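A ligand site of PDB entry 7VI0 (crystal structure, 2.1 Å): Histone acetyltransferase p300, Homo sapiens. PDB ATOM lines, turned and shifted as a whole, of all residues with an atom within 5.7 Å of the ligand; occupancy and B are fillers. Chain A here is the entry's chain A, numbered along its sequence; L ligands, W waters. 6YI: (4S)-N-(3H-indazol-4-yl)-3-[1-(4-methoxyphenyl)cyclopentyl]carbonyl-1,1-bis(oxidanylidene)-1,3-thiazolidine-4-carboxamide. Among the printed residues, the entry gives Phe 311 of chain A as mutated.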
ATOM      1  N   PHE A 218     -22.736 -31.614   2.886  1.00  0.00           N
ATOM      2  CA  PHE A 218     -22.034 -31.200   4.085  1.00  0.00           C
ATOM      3  C   PHE A 218     -20.922 -30.227   3.716  1.00  0.00           C
ATOM      4  O   PHE A 218     -20.231 -30.423   2.713  1.00  0.00           O
ATOM      5  CB  PHE A 218     -21.466 -32.420   4.816  1.00  0.00           C
ATOM      6  CG  PHE A 218     -20.646 -32.073   6.034  1.00  0.00           C
ATOM      7  CD1 PHE A 218     -21.261 -31.890   7.269  1.00  0.00           C
ATOM      8  CD2 PHE A 218     -19.268 -31.927   5.953  1.00  0.00           C
ATOM      9  CE1 PHE A 218     -20.511 -31.574   8.389  1.00  0.00           C
ATOM     10  CE2 PHE A 218     -18.523 -31.604   7.069  1.00  0.00           C
ATOM     11  CZ  PHE A 218     -19.141 -31.434   8.285  1.00  0.00           C
ATOM     12  N   LEU A 242     -20.163 -25.026  10.402  1.00  0.00           N
ATOM     13  CA  LEU A 242     -20.623 -26.292   9.834  1.00  0.00           C
ATOM     14  C   LEU A 242     -22.000 -26.077   9.212  1.00  0.00           C
ATOM     15  O   LEU A 242     -22.776 -25.237   9.676  1.00  0.00           O
ATOM     16  CB  LEU A 242     -20.740 -27.397  10.893  1.00  0.00           C
ATOM     17  CG  LEU A 242     -19.567 -27.743  11.797  1.00  0.00           C
ATOM     18  CD1 LEU A 242     -20.033 -28.580  12.974  1.00  0.00           C
ATOM     19  CD2 LEU A 242     -18.552 -28.515  11.021  1.00  0.00           C
ATOM     20  N   ASP A 243     -22.296 -26.840   8.162  1.00  0.00           N
ATOM     21  CA  ASP A 243     -23.617 -26.768   7.552  1.00  0.00           C
ATOM     22  C   ASP A 243     -23.894 -28.059   6.800  1.00  0.00           C
ATOM     23  O   ASP A 243     -22.973 -28.824   6.503  1.00  0.00           O
ATOM     24  CB  ASP A 243     -23.746 -25.560   6.625  1.00  0.00           C
ATOM     25  CG  ASP A 243     -25.176 -25.080   6.470  1.00  0.00           C
ATOM     26  OD1 ASP A 243     -26.091 -25.706   7.071  1.00  0.00           O
ATOM     27  OD2 ASP A 243     -25.396 -24.076   5.755  1.00  0.00           O
ATOM     28  N   SER A 244     -25.163 -28.288   6.497  1.00  0.00           N
ATOM     29  CA  SER A 244     -25.592 -29.523   5.868  1.00  0.00           C
ATOM     30  C   SER A 244     -26.883 -29.306   5.088  1.00  0.00           C
ATOM     31  O   SER A 244     -27.667 -28.397   5.395  1.00  0.00           O
ATOM     32  CB  SER A 244     -25.795 -30.636   6.904  1.00  0.00           C
ATOM     33  OG  SER A 244     -26.861 -30.335   7.773  1.00  0.00           O
ATOM     34  N   TYR A 258     -22.142 -37.502   9.442  1.00  0.00           N
ATOM     35  CA  TYR A 258     -21.633 -36.237   9.945  1.00  0.00           C
ATOM     36  C   TYR A 258     -20.615 -36.463  11.057  1.00  0.00           C
ATOM     37  O   TYR A 258     -19.535 -35.872  11.063  1.00  0.00           O
ATOM     38  CB  TYR A 258     -22.759 -35.349  10.478  1.00  0.00           C
ATOM     39  CG  TYR A 258     -23.824 -34.925   9.502  1.00  0.00           C
ATOM     40  CD1 TYR A 258     -23.521 -34.665   8.172  1.00  0.00           C
ATOM     41  CD2 TYR A 258     -25.135 -34.763   9.909  1.00  0.00           C
ATOM     42  CE1 TYR A 258     -24.507 -34.266   7.276  1.00  0.00           C
ATOM     43  CE2 TYR A 258     -26.127 -34.377   9.039  1.00  0.00           C
ATOM     44  CZ  TYR A 258     -25.807 -34.128   7.719  1.00  0.00           C
ATOM     45  OH  TYR A 258     -26.801 -33.738   6.858  1.00  0.00           O
ATOM     46  N   LEU A 262     -16.471 -35.527  11.272  1.00  0.00           N
ATOM     47  CA  LEU A 262     -15.895 -34.711  12.334  1.00  0.00           C
ATOM     48  C   LEU A 262     -14.860 -35.499  13.135  1.00  0.00           C
ATOM     49  O   LEU A 262     -13.795 -34.969  13.459  1.00  0.00           O
ATOM     50  CB  LEU A 262     -17.003 -34.171  13.232  1.00  0.00           C
ATOM     51  CG  LEU A 262     -17.867 -33.088  12.599  1.00  0.00           C
ATOM     52  CD1 LEU A 262     -18.917 -32.555  13.563  1.00  0.00           C
ATOM     53  CD2 LEU A 262     -16.993 -31.944  12.085  1.00  0.00           C
ATOM     54  N   CYS A 282     -22.957 -23.114  18.217  1.00  0.00           N
ATOM     55  CA  CYS A 282     -23.656 -21.845  18.004  1.00  0.00           C
ATOM     56  C   CYS A 282     -24.617 -21.983  16.833  1.00  0.00           C
ATOM     57  O   CYS A 282     -24.186 -21.944  15.661  1.00  0.00           O
ATOM     58  CB  CYS A 282     -22.648 -20.738  17.760  1.00  0.00           C
ATOM     59  SG  CYS A 282     -23.278 -19.220  17.002  1.00  0.00           S
ATOM     60  N   PRO A 283     -25.911 -22.149  17.084  1.00  0.00           N
ATOM     61  CA  PRO A 283     -26.875 -22.204  15.988  1.00  0.00           C
ATOM     62  C   PRO A 283     -26.907 -20.896  15.227  1.00  0.00           C
ATOM     63  O   PRO A 283     -26.789 -19.820  15.825  1.00  0.00           O
ATOM     64  CB  PRO A 283     -28.212 -22.473  16.703  1.00  0.00           C
ATOM     65  CG  PRO A 283     -27.835 -23.046  18.020  1.00  0.00           C
ATOM     66  CD  PRO A 283     -26.538 -22.400  18.395  1.00  0.00           C
ATOM     67  N   PRO A 284     -27.084 -20.949  13.907  1.00  0.00           N
ATOM     68  CA  PRO A 284     -27.235 -19.714  13.132  1.00  0.00           C
ATOM     69  C   PRO A 284     -28.565 -19.042  13.464  1.00  0.00           C
ATOM     70  O   PRO A 284     -29.491 -19.641  13.993  1.00  0.00           O
ATOM     71  CB  PRO A 284     -27.192 -20.191  11.680  1.00  0.00           C
ATOM     72  CG  PRO A 284     -27.451 -21.660  11.726  1.00  0.00           C
ATOM     73  CD  PRO A 284     -26.957 -22.136  13.057  1.00  0.00           C
ATOM     74  N   SER A 285     -28.627 -17.754  13.122  1.00  0.00           N
ATOM     75  CA  SER A 285     -29.879 -17.020  13.256  1.00  0.00           C
ATOM     76  C   SER A 285     -30.944 -17.607  12.346  1.00  0.00           C
ATOM     77  O   SER A 285     -30.643 -18.231  11.318  1.00  0.00           O
ATOM     78  CB  SER A 285     -29.667 -15.544  12.900  1.00  0.00           C
ATOM     79  OG  SER A 285     -29.617 -15.361  11.496  1.00  0.00           O
ATOM     80  N   GLY A 287     -33.496 -18.343   9.583  1.00  0.00           N
ATOM     81  CA  GLY A 287     -33.353 -18.057   8.161  1.00  0.00           C
ATOM     82  C   GLY A 287     -32.821 -19.285   7.458  1.00  0.00           C
ATOM     83  O   GLY A 287     -32.599 -20.306   8.102  1.00  0.00           O
ATOM     84  N   ASP A 288     -32.637 -19.224   6.137  1.00  0.00           N
ATOM     85  CA  ASP A 288     -32.210 -20.400   5.380  1.00  0.00           C
ATOM     86  C   ASP A 288     -30.846 -20.268   4.711  1.00  0.00           C
ATOM     87  O   ASP A 288     -30.493 -21.124   3.892  1.00  0.00           O
ATOM     88  CB  ASP A 288     -33.260 -20.779   4.335  1.00  0.00           C
ATOM     89  CG  ASP A 288     -33.711 -19.598   3.497  1.00  0.00           C
ATOM     90  OD1 ASP A 288     -32.991 -18.584   3.438  1.00  0.00           O
ATOM     91  OD2 ASP A 288     -34.804 -19.687   2.889  1.00  0.00           O
ATOM     92  N   ASP A 289     -30.046 -19.241   5.031  1.00  0.00           N
ATOM     93  CA  ASP A 289     -28.726 -19.075   4.437  1.00  0.00           C
ATOM     94  C   ASP A 289     -27.639 -19.095   5.511  1.00  0.00           C
ATOM     95  O   ASP A 289     -27.625 -18.223   6.395  1.00  0.00           O
ATOM     96  CB  ASP A 289     -28.621 -17.747   3.672  1.00  0.00           C
ATOM     97  CG  ASP A 289     -29.536 -17.676   2.467  1.00  0.00           C
ATOM     98  OD1 ASP A 289     -30.198 -18.683   2.144  1.00  0.00           O
ATOM     99  OD2 ASP A 289     -29.597 -16.595   1.844  1.00  0.00           O
ATOM    100  N   TYR A 290     -26.775 -20.105   5.476  1.00  0.00           N
ATOM    101  CA  TYR A 290     -25.591 -20.097   6.340  1.00  0.00           C
ATOM    102  C   TYR A 290     -24.312 -20.313   5.529  1.00  0.00           C
ATOM    103  O   TYR A 290     -23.517 -19.380   5.312  1.00  0.00           O
ATOM    104  CB  TYR A 290     -25.741 -21.165   7.406  1.00  0.00           C
ATOM    105  CG  TYR A 290     -24.772 -21.080   8.546  1.00  0.00           C
ATOM    106  CD1 TYR A 290     -24.483 -19.858   9.151  1.00  0.00           C
ATOM    107  CD2 TYR A 290     -24.162 -22.211   9.046  1.00  0.00           C
ATOM    108  CE1 TYR A 290     -23.600 -19.777  10.211  1.00  0.00           C
ATOM    109  CE2 TYR A 290     -23.278 -22.151  10.093  1.00  0.00           C
ATOM    110  CZ  TYR A 290     -22.998 -20.934  10.676  1.00  0.00           C
ATOM    111  OH  TYR A 290     -22.119 -20.886  11.727  1.00  0.00           O
ATOM    112  N   PHE A 292     -24.890 -22.989   2.824  1.00  0.00           N
ATOM    113  CA  PHE A 292     -25.724 -23.377   1.700  1.00  0.00           C
ATOM    114  C   PHE A 292     -26.902 -22.412   1.640  1.00  0.00           C
ATOM    115  O   PHE A 292     -27.510 -22.102   2.673  1.00  0.00           O
ATOM    116  CB  PHE A 292     -26.224 -24.814   1.865  1.00  0.00           C
ATOM    117  CG  PHE A 292     -25.131 -25.848   1.863  1.00  0.00           C
ATOM    118  CD1 PHE A 292     -24.560 -26.245   0.677  1.00  0.00           C
ATOM    119  CD2 PHE A 292     -24.685 -26.412   3.049  1.00  0.00           C
ATOM    120  CE1 PHE A 292     -23.545 -27.200   0.662  1.00  0.00           C
ATOM    121  CE2 PHE A 292     -23.681 -27.369   3.043  1.00  0.00           C
ATOM    122  CZ  PHE A 292     -23.112 -27.761   1.843  1.00  0.00           C
ATOM    123  N   HIS A 295     -31.919 -23.434   2.567  1.00  0.00           N
ATOM    124  CA  HIS A 295     -32.116 -24.768   3.126  1.00  0.00           C
ATOM    125  C   HIS A 295     -33.556 -25.249   2.897  1.00  0.00           C
ATOM    126  O   HIS A 295     -34.472 -24.454   2.683  1.00  0.00           O
ATOM    127  CB  HIS A 295     -31.814 -24.748   4.621  1.00  0.00           C
ATOM    128  CG  HIS A 295     -30.356 -24.715   4.942  1.00  0.00           C
ATOM    129  ND1 HIS A 295     -29.585 -23.579   4.786  1.00  0.00           N
ATOM    130  CD2 HIS A 295     -29.510 -25.670   5.399  1.00  0.00           C
ATOM    131  CE1 HIS A 295     -28.348 -23.832   5.147  1.00  0.00           C
ATOM    132  NE2 HIS A 295     -28.276 -25.098   5.516  1.00  0.00           N
ATOM    133  N   PRO A 296     -33.769 -26.575   2.927  1.00  0.00           N
ATOM    134  CA  PRO A 296     -35.139 -27.106   2.786  1.00  0.00           C
ATOM    135  C   PRO A 296     -36.051 -26.585   3.885  1.00  0.00           C
ATOM    136  O   PRO A 296     -35.627 -26.491   5.054  1.00  0.00           O
ATOM    137  CB  PRO A 296     -34.938 -28.625   2.897  1.00  0.00           C
ATOM    138  CG  PRO A 296     -33.510 -28.858   2.568  1.00  0.00           C
ATOM    139  CD  PRO A 296     -32.777 -27.642   3.046  1.00  0.00           C
ATOM    140  N   GLN A 299     -36.049 -28.679   6.993  1.00  0.00           N
ATOM    141  CA  GLN A 299     -34.797 -28.843   7.726  1.00  0.00           C
ATOM    142  C   GLN A 299     -34.674 -27.706   8.740  1.00  0.00           C
ATOM    143  O   GLN A 299     -34.610 -26.539   8.364  1.00  0.00           O
ATOM    144  CB  GLN A 299     -33.589 -28.861   6.795  1.00  0.00           C
ATOM    145  CG  GLN A 299     -32.273 -29.101   7.535  1.00  0.00           C
ATOM    146  CD  GLN A 299     -31.059 -29.151   6.632  1.00  0.00           C
ATOM    147  OE1 GLN A 299     -31.170 -29.227   5.410  1.00  0.00           O
ATOM    148  NE2 GLN A 299     -29.877 -29.100   7.249  1.00  0.00           N
ATOM    149  N   LYS A 300     -34.653 -28.069  10.018  1.00  0.00           N
ATOM    150  CA  LYS A 300     -34.714 -27.100  11.109  1.00  0.00           C
ATOM    151  C   LYS A 300     -33.328 -26.859  11.713  1.00  0.00           C
ATOM    152  O   LYS A 300     -32.500 -27.773  11.784  1.00  0.00           O
ATOM    153  CB  LYS A 300     -35.677 -27.575  12.195  1.00  0.00           C
ATOM    154  CG  LYS A 300     -37.073 -27.866  11.668  1.00  0.00           C
ATOM    155  CD  LYS A 300     -37.637 -26.674  10.927  1.00  0.00           C
ATOM    156  CE  LYS A 300     -38.896 -27.028  10.151  1.00  0.00           C
ATOM    157  NZ  LYS A 300     -39.583 -25.818   9.638  1.00  0.00           N
ATOM    158  N   ILE A 301     -33.088 -25.618  12.136  1.00  0.00           N
ATOM    159  CA  ILE A 301     -31.904 -25.295  12.927  1.00  0.00           C
ATOM    160  C   ILE A 301     -32.111 -25.837  14.343  1.00  0.00           C
ATOM    161  O   ILE A 301     -33.135 -25.529  14.972  1.00  0.00           O
ATOM    162  CB  ILE A 301     -31.640 -23.780  12.953  1.00  0.00           C
ATOM    163  CG1 ILE A 301     -31.255 -23.271  11.559  1.00  0.00           C
ATOM    164  CG2 ILE A 301     -30.544 -23.439  13.960  1.00  0.00           C
ATOM    165  CD1 ILE A 301     -31.506 -21.799  11.351  1.00  0.00           C
ATOM    166  N   PRO A 302     -31.204 -26.659  14.861  1.00  0.00           N
ATOM    167  CA  PRO A 302     -31.384 -27.182  16.219  1.00  0.00           C
ATOM    168  C   PRO A 302     -31.305 -26.070  17.254  1.00  0.00           C
ATOM    169  O   PRO A 302     -30.570 -25.096  17.115  1.00  0.00           O
ATOM    170  CB  PRO A 302     -30.223 -28.165  16.373  1.00  0.00           C
ATOM    171  CG  PRO A 302     -29.175 -27.632  15.478  1.00  0.00           C
ATOM    172  CD  PRO A 302     -29.912 -27.061  14.284  1.00  0.00           C
ATOM    173  N   ARG A 306     -30.058 -29.195  22.091  1.00  0.00           N
ATOM    174  CA  ARG A 306     -29.995 -30.367  21.215  1.00  0.00           C
ATOM    175  C   ARG A 306     -28.719 -30.371  20.377  1.00  0.00           C
ATOM    176  O   ARG A 306     -28.187 -31.445  20.081  1.00  0.00           O
ATOM    177  CB  ARG A 306     -31.257 -30.443  20.370  1.00  0.00           C
ATOM    178  CG  ARG A 306     -32.465 -30.831  21.221  1.00  0.00           C
ATOM    179  CD  ARG A 306     -33.662 -31.270  20.398  1.00  0.00           C
ATOM    180  NE  ARG A 306     -33.429 -32.540  19.741  1.00  0.00           N
ATOM    181  CZ  ARG A 306     -33.284 -32.676  18.427  1.00  0.00           C
ATOM    182  NH1 ARG A 306     -33.345 -31.641  17.620  1.00  0.00           N
ATOM    183  NH2 ARG A 306     -33.070 -33.881  17.916  1.00  0.00           N
ATOM    184  N   LEU A 307     -28.247 -29.192  19.956  1.00  0.00           N
ATOM    185  CA  LEU A 307     -26.964 -29.137  19.253  1.00  0.00           C
ATOM    186  C   LEU A 307     -25.830 -29.576  20.164  1.00  0.00           C
ATOM    187  O   LEU A 307     -24.929 -30.315  19.737  1.00  0.00           O
ATOM    188  CB  LEU A 307     -26.722 -27.722  18.727  1.00  0.00           C
ATOM    189  CG  LEU A 307     -25.388 -27.469  18.008  1.00  0.00           C
ATOM    190  CD1 LEU A 307     -25.260 -28.384  16.798  1.00  0.00           C
ATOM    191  CD2 LEU A 307     -25.258 -26.006  17.598  1.00  0.00           C
ATOM    192  N   TRP A 310     -25.739 -33.234  20.483  1.00  0.00           N
ATOM    193  CA  TRP A 310     -25.217 -33.762  19.227  1.00  0.00           C
ATOM    194  C   TRP A 310     -23.690 -33.767  19.211  1.00  0.00           C
ATOM    195  O   TRP A 310     -23.077 -34.748  18.784  1.00  0.00           O
ATOM    196  CB  TRP A 310     -25.778 -32.934  18.072  1.00  0.00           C
ATOM    197  CG  TRP A 310     -25.509 -33.432  16.684  1.00  0.00           C
ATOM    198  CD1 TRP A 310     -26.317 -34.246  15.938  1.00  0.00           C
ATOM    199  CD2 TRP A 310     -24.388 -33.117  15.852  1.00  0.00           C
ATOM    200  NE1 TRP A 310     -25.755 -34.458  14.701  1.00  0.00           N
ATOM    201  CE2 TRP A 310     -24.569 -33.784  14.623  1.00  0.00           C
ATOM    202  CE3 TRP A 310     -23.233 -32.346  16.027  1.00  0.00           C
ATOM    203  CZ2 TRP A 310     -23.641 -33.701  13.577  1.00  0.00           C
ATOM    204  CZ3 TRP A 310     -22.316 -32.264  14.989  1.00  0.00           C
ATOM    205  CH2 TRP A 310     -22.529 -32.938  13.777  1.00  0.00           C
ATOM    206  N   PHE A 311     -23.068 -32.680  19.679  1.00  0.00           N
ATOM    207  CA  PHE A 311     -21.610 -32.649  19.763  1.00  0.00           C
ATOM    208  C   PHE A 311     -21.087 -33.588  20.832  1.00  0.00           C
ATOM    209  O   PHE A 311     -20.022 -34.208  20.648  1.00  0.00           O
ATOM    210  CB  PHE A 311     -21.137 -31.217  20.022  1.00  0.00           C
ATOM    211  CG  PHE A 311     -21.081 -30.359  18.796  1.00  0.00           C
ATOM    212  CD1 PHE A 311     -20.252 -30.695  17.737  1.00  0.00           C
ATOM    213  CD2 PHE A 311     -21.859 -29.223  18.686  1.00  0.00           C
ATOM    214  CE1 PHE A 311     -20.202 -29.915  16.600  1.00  0.00           C
ATOM    215  CE2 PHE A 311     -21.816 -28.432  17.553  1.00  0.00           C
ATOM    216  CZ  PHE A 311     -20.985 -28.771  16.508  1.00  0.00           C
HETATM  217  N   6YI L   1     -26.089 -27.573  11.754  1.00  0.00           N
HETATM  218  CA  6YI L   1     -26.297 -26.314  10.917  1.00  0.00           C
HETATM  219  C   6YI L   1     -27.610 -25.931  10.647  1.00  0.00           C
HETATM  220  O   6YI L   1     -28.420 -25.784  11.546  1.00  0.00           O
HETATM  221  CB  6YI L   1     -25.517 -25.199  11.612  1.00  0.00           C
HETATM  222  CAF 6YI L   1     -29.129 -25.281   9.019  1.00  0.00           C
HETATM  223  CAG 6YI L   1     -30.211 -26.135   9.026  1.00  0.00           C
HETATM  224  CAH 6YI L   1     -31.440 -25.647   8.620  1.00  0.00           C
HETATM  225  CAI 6YI L   1     -31.541 -24.327   8.218  1.00  0.00           C
HETATM  226  CAJ 6YI L   1     -30.455 -23.563   8.229  1.00  0.00           C
HETATM  227  CAK 6YI L   1     -29.293 -24.032   8.619  1.00  0.00           C
HETATM  228  CAL 6YI L   1     -28.489 -22.998   8.496  1.00  0.00           C
HETATM  229  CAQ 6YI L   1     -26.197 -27.269  13.230  1.00  0.00           C
HETATM  230  CAT 6YI L   1     -25.865 -28.697  11.028  1.00  0.00           C
HETATM  231  CAV 6YI L   1     -25.626 -30.044  11.754  1.00  0.00           C
HETATM  232  CAW 6YI L   1     -26.658 -30.400  12.631  1.00  0.00           C
HETATM  233  CAX 6YI L   1     -27.975 -30.388  12.196  1.00  0.00           C
HETATM  234  CAY 6YI L   1     -28.998 -30.718  13.064  1.00  0.00           C
HETATM  235  CAZ 6YI L   1     -28.717 -31.058  14.384  1.00  0.00           C
HETATM  236  CBA 6YI L   1     -27.404 -31.062  14.815  1.00  0.00           C
HETATM  237  CBB 6YI L   1     -26.381 -30.731  13.947  1.00  0.00           C
HETATM  238  CBD 6YI L   1     -29.245 -31.816  16.494  1.00  0.00           C
HETATM  239  CBE 6YI L   1     -25.447 -31.150  10.758  1.00  0.00           C
HETATM  240  CBF 6YI L   1     -23.957 -31.295  10.499  1.00  0.00           C
HETATM  241  CBG 6YI L   1     -23.317 -30.204  11.299  1.00  0.00           C
HETATM  242  CBH 6YI L   1     -24.268 -30.026  12.438  1.00  0.00           C
HETATM  243  NAE 6YI L   1     -27.891 -25.657   9.367  1.00  0.00           N
HETATM  244  NAM 6YI L   1     -29.226 -21.993   8.048  1.00  0.00           N
HETATM  245  NAN 6YI L   1     -30.267 -22.294   7.912  1.00  0.00           N
HETATM  246  OAR 6YI L   1     -23.720 -26.257  13.639  1.00  0.00           O
HETATM  247  OAS 6YI L   1     -25.682 -24.941  14.474  1.00  0.00           O
HETATM  248  OAU 6YI L   1     -25.850 -28.650   9.811  1.00  0.00           O
HETATM  249  OBC 6YI L   1     -29.727 -31.387  15.222  1.00  0.00           O
HETATM  250  SAP 6YI L   1     -25.151 -25.827  13.381  1.00  0.00           S
HETATM  251  O   HOH W   1     -23.425 -22.750  13.240  1.00  0.00           O
HETATM  252  O   HOH W   2     -29.483 -18.842   8.825  1.00  0.00           O
HETATM  253  O   HOH W   3     -30.665 -29.374  10.438  1.00  0.00           O
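An oxygen (OAU) of the ligand lies within hydrogen-bond range of the backbone NH (N) of Ser 244 (3.4 Å).
An oxygen (OAU) of the ligand is in hydrogen-bond range of the side-chain hydroxyl (OG) of Ser 244 (2.8 Å).
The side-chain carboxylate of Asp 243 is in hydrogen-bond range of a nitrogen (NAE) of the ligand (2.9 Å).
A nitrogen (NAN) of the ligand is in hydrogen-bond range of the backbone carbonyl oxygen of Gly 287, at 3.1 Å.
ND1 of His 295 lies within hydrogen-bond range of NAN of the ligand (3.4 Å).
The backbone carbonyl oxygen of Ser 244 sits at hydrogen-bond distance from the side-chain amide nitrogen of Gln 299 (3.0 Å).
NE2 of His 295 lies close to O of Ser 244 (3.4 Å).
The side-chain carboxylate (OD1) of Asp 243 sits at hydrogen-bond distance from a ring nitrogen (NE2) of His 295.
The side-chain carboxylate (OD2) of Asp 243 lies within hydrogen-bond range of the backbone NH (N) of Phe 292 (3.2 Å).
The backbone carbonyl oxygen of Asp 288 is in hydrogen-bond range of a ring nitrogen (ND1) of His 295, at 2.8 Å.
A ring nitrogen (ND1) of His 295 sits close to the backbone carbonyl oxygen (O) of Phe 292, 3.3 Å away.
Residues that only touch the ligand: Leu 242 (3.4 Å), Tyr 258 (3.7 Å), Cys 282 (3.6 Å), Pro 283 (3.3 Å), Pro 284 (3.4 Å), Asp 288 (3.7 Å), Tyr 290 (3.5 Å), Gln 299 (3.3 Å), Lys 300 (3.8 Å), Ile 301 (3.4 Å), Pro 302 (3.4 Å), Arg 306 (3.8 Å), Leu 307 (3.3 Å) and Trp 310 (3.5 Å).
Hydrophobic or aromatic side chains within 4 Å of the ligand: Leu 242, Tyr 258, Pro 284, Tyr 290, His 295, Ile 301, Pro 302, Leu 307 and Trp 310.
18 residues have an atom within 4 Å of the ligand: Leu 242, Asp 243, Ser 244, Tyr 258, Cys 282, Pro 283, Pro 284, Gly 287, Asp 288, Tyr 290, His 295, Gln 299, Lys 300, Ile 301, Pro 302, Arg 306, Leu 307 and Trp 310.
Water W2 lies within hydrogen-bond range of O of Ser 285 (2.8 Å), O of Asp 289 (3.1 Å) and NAM of the ligand (3.3 Å).
Water W3 bridges O of Lys 300 (2.8 Å) and NE2 of Gln 299 (3.3 Å).
Water W1 lies within hydrogen-bond range of the backbone carbonyl oxygen of Cys 282, the side-chain hydroxyl of Tyr 290 and an oxygen (OAS) of the ligand.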
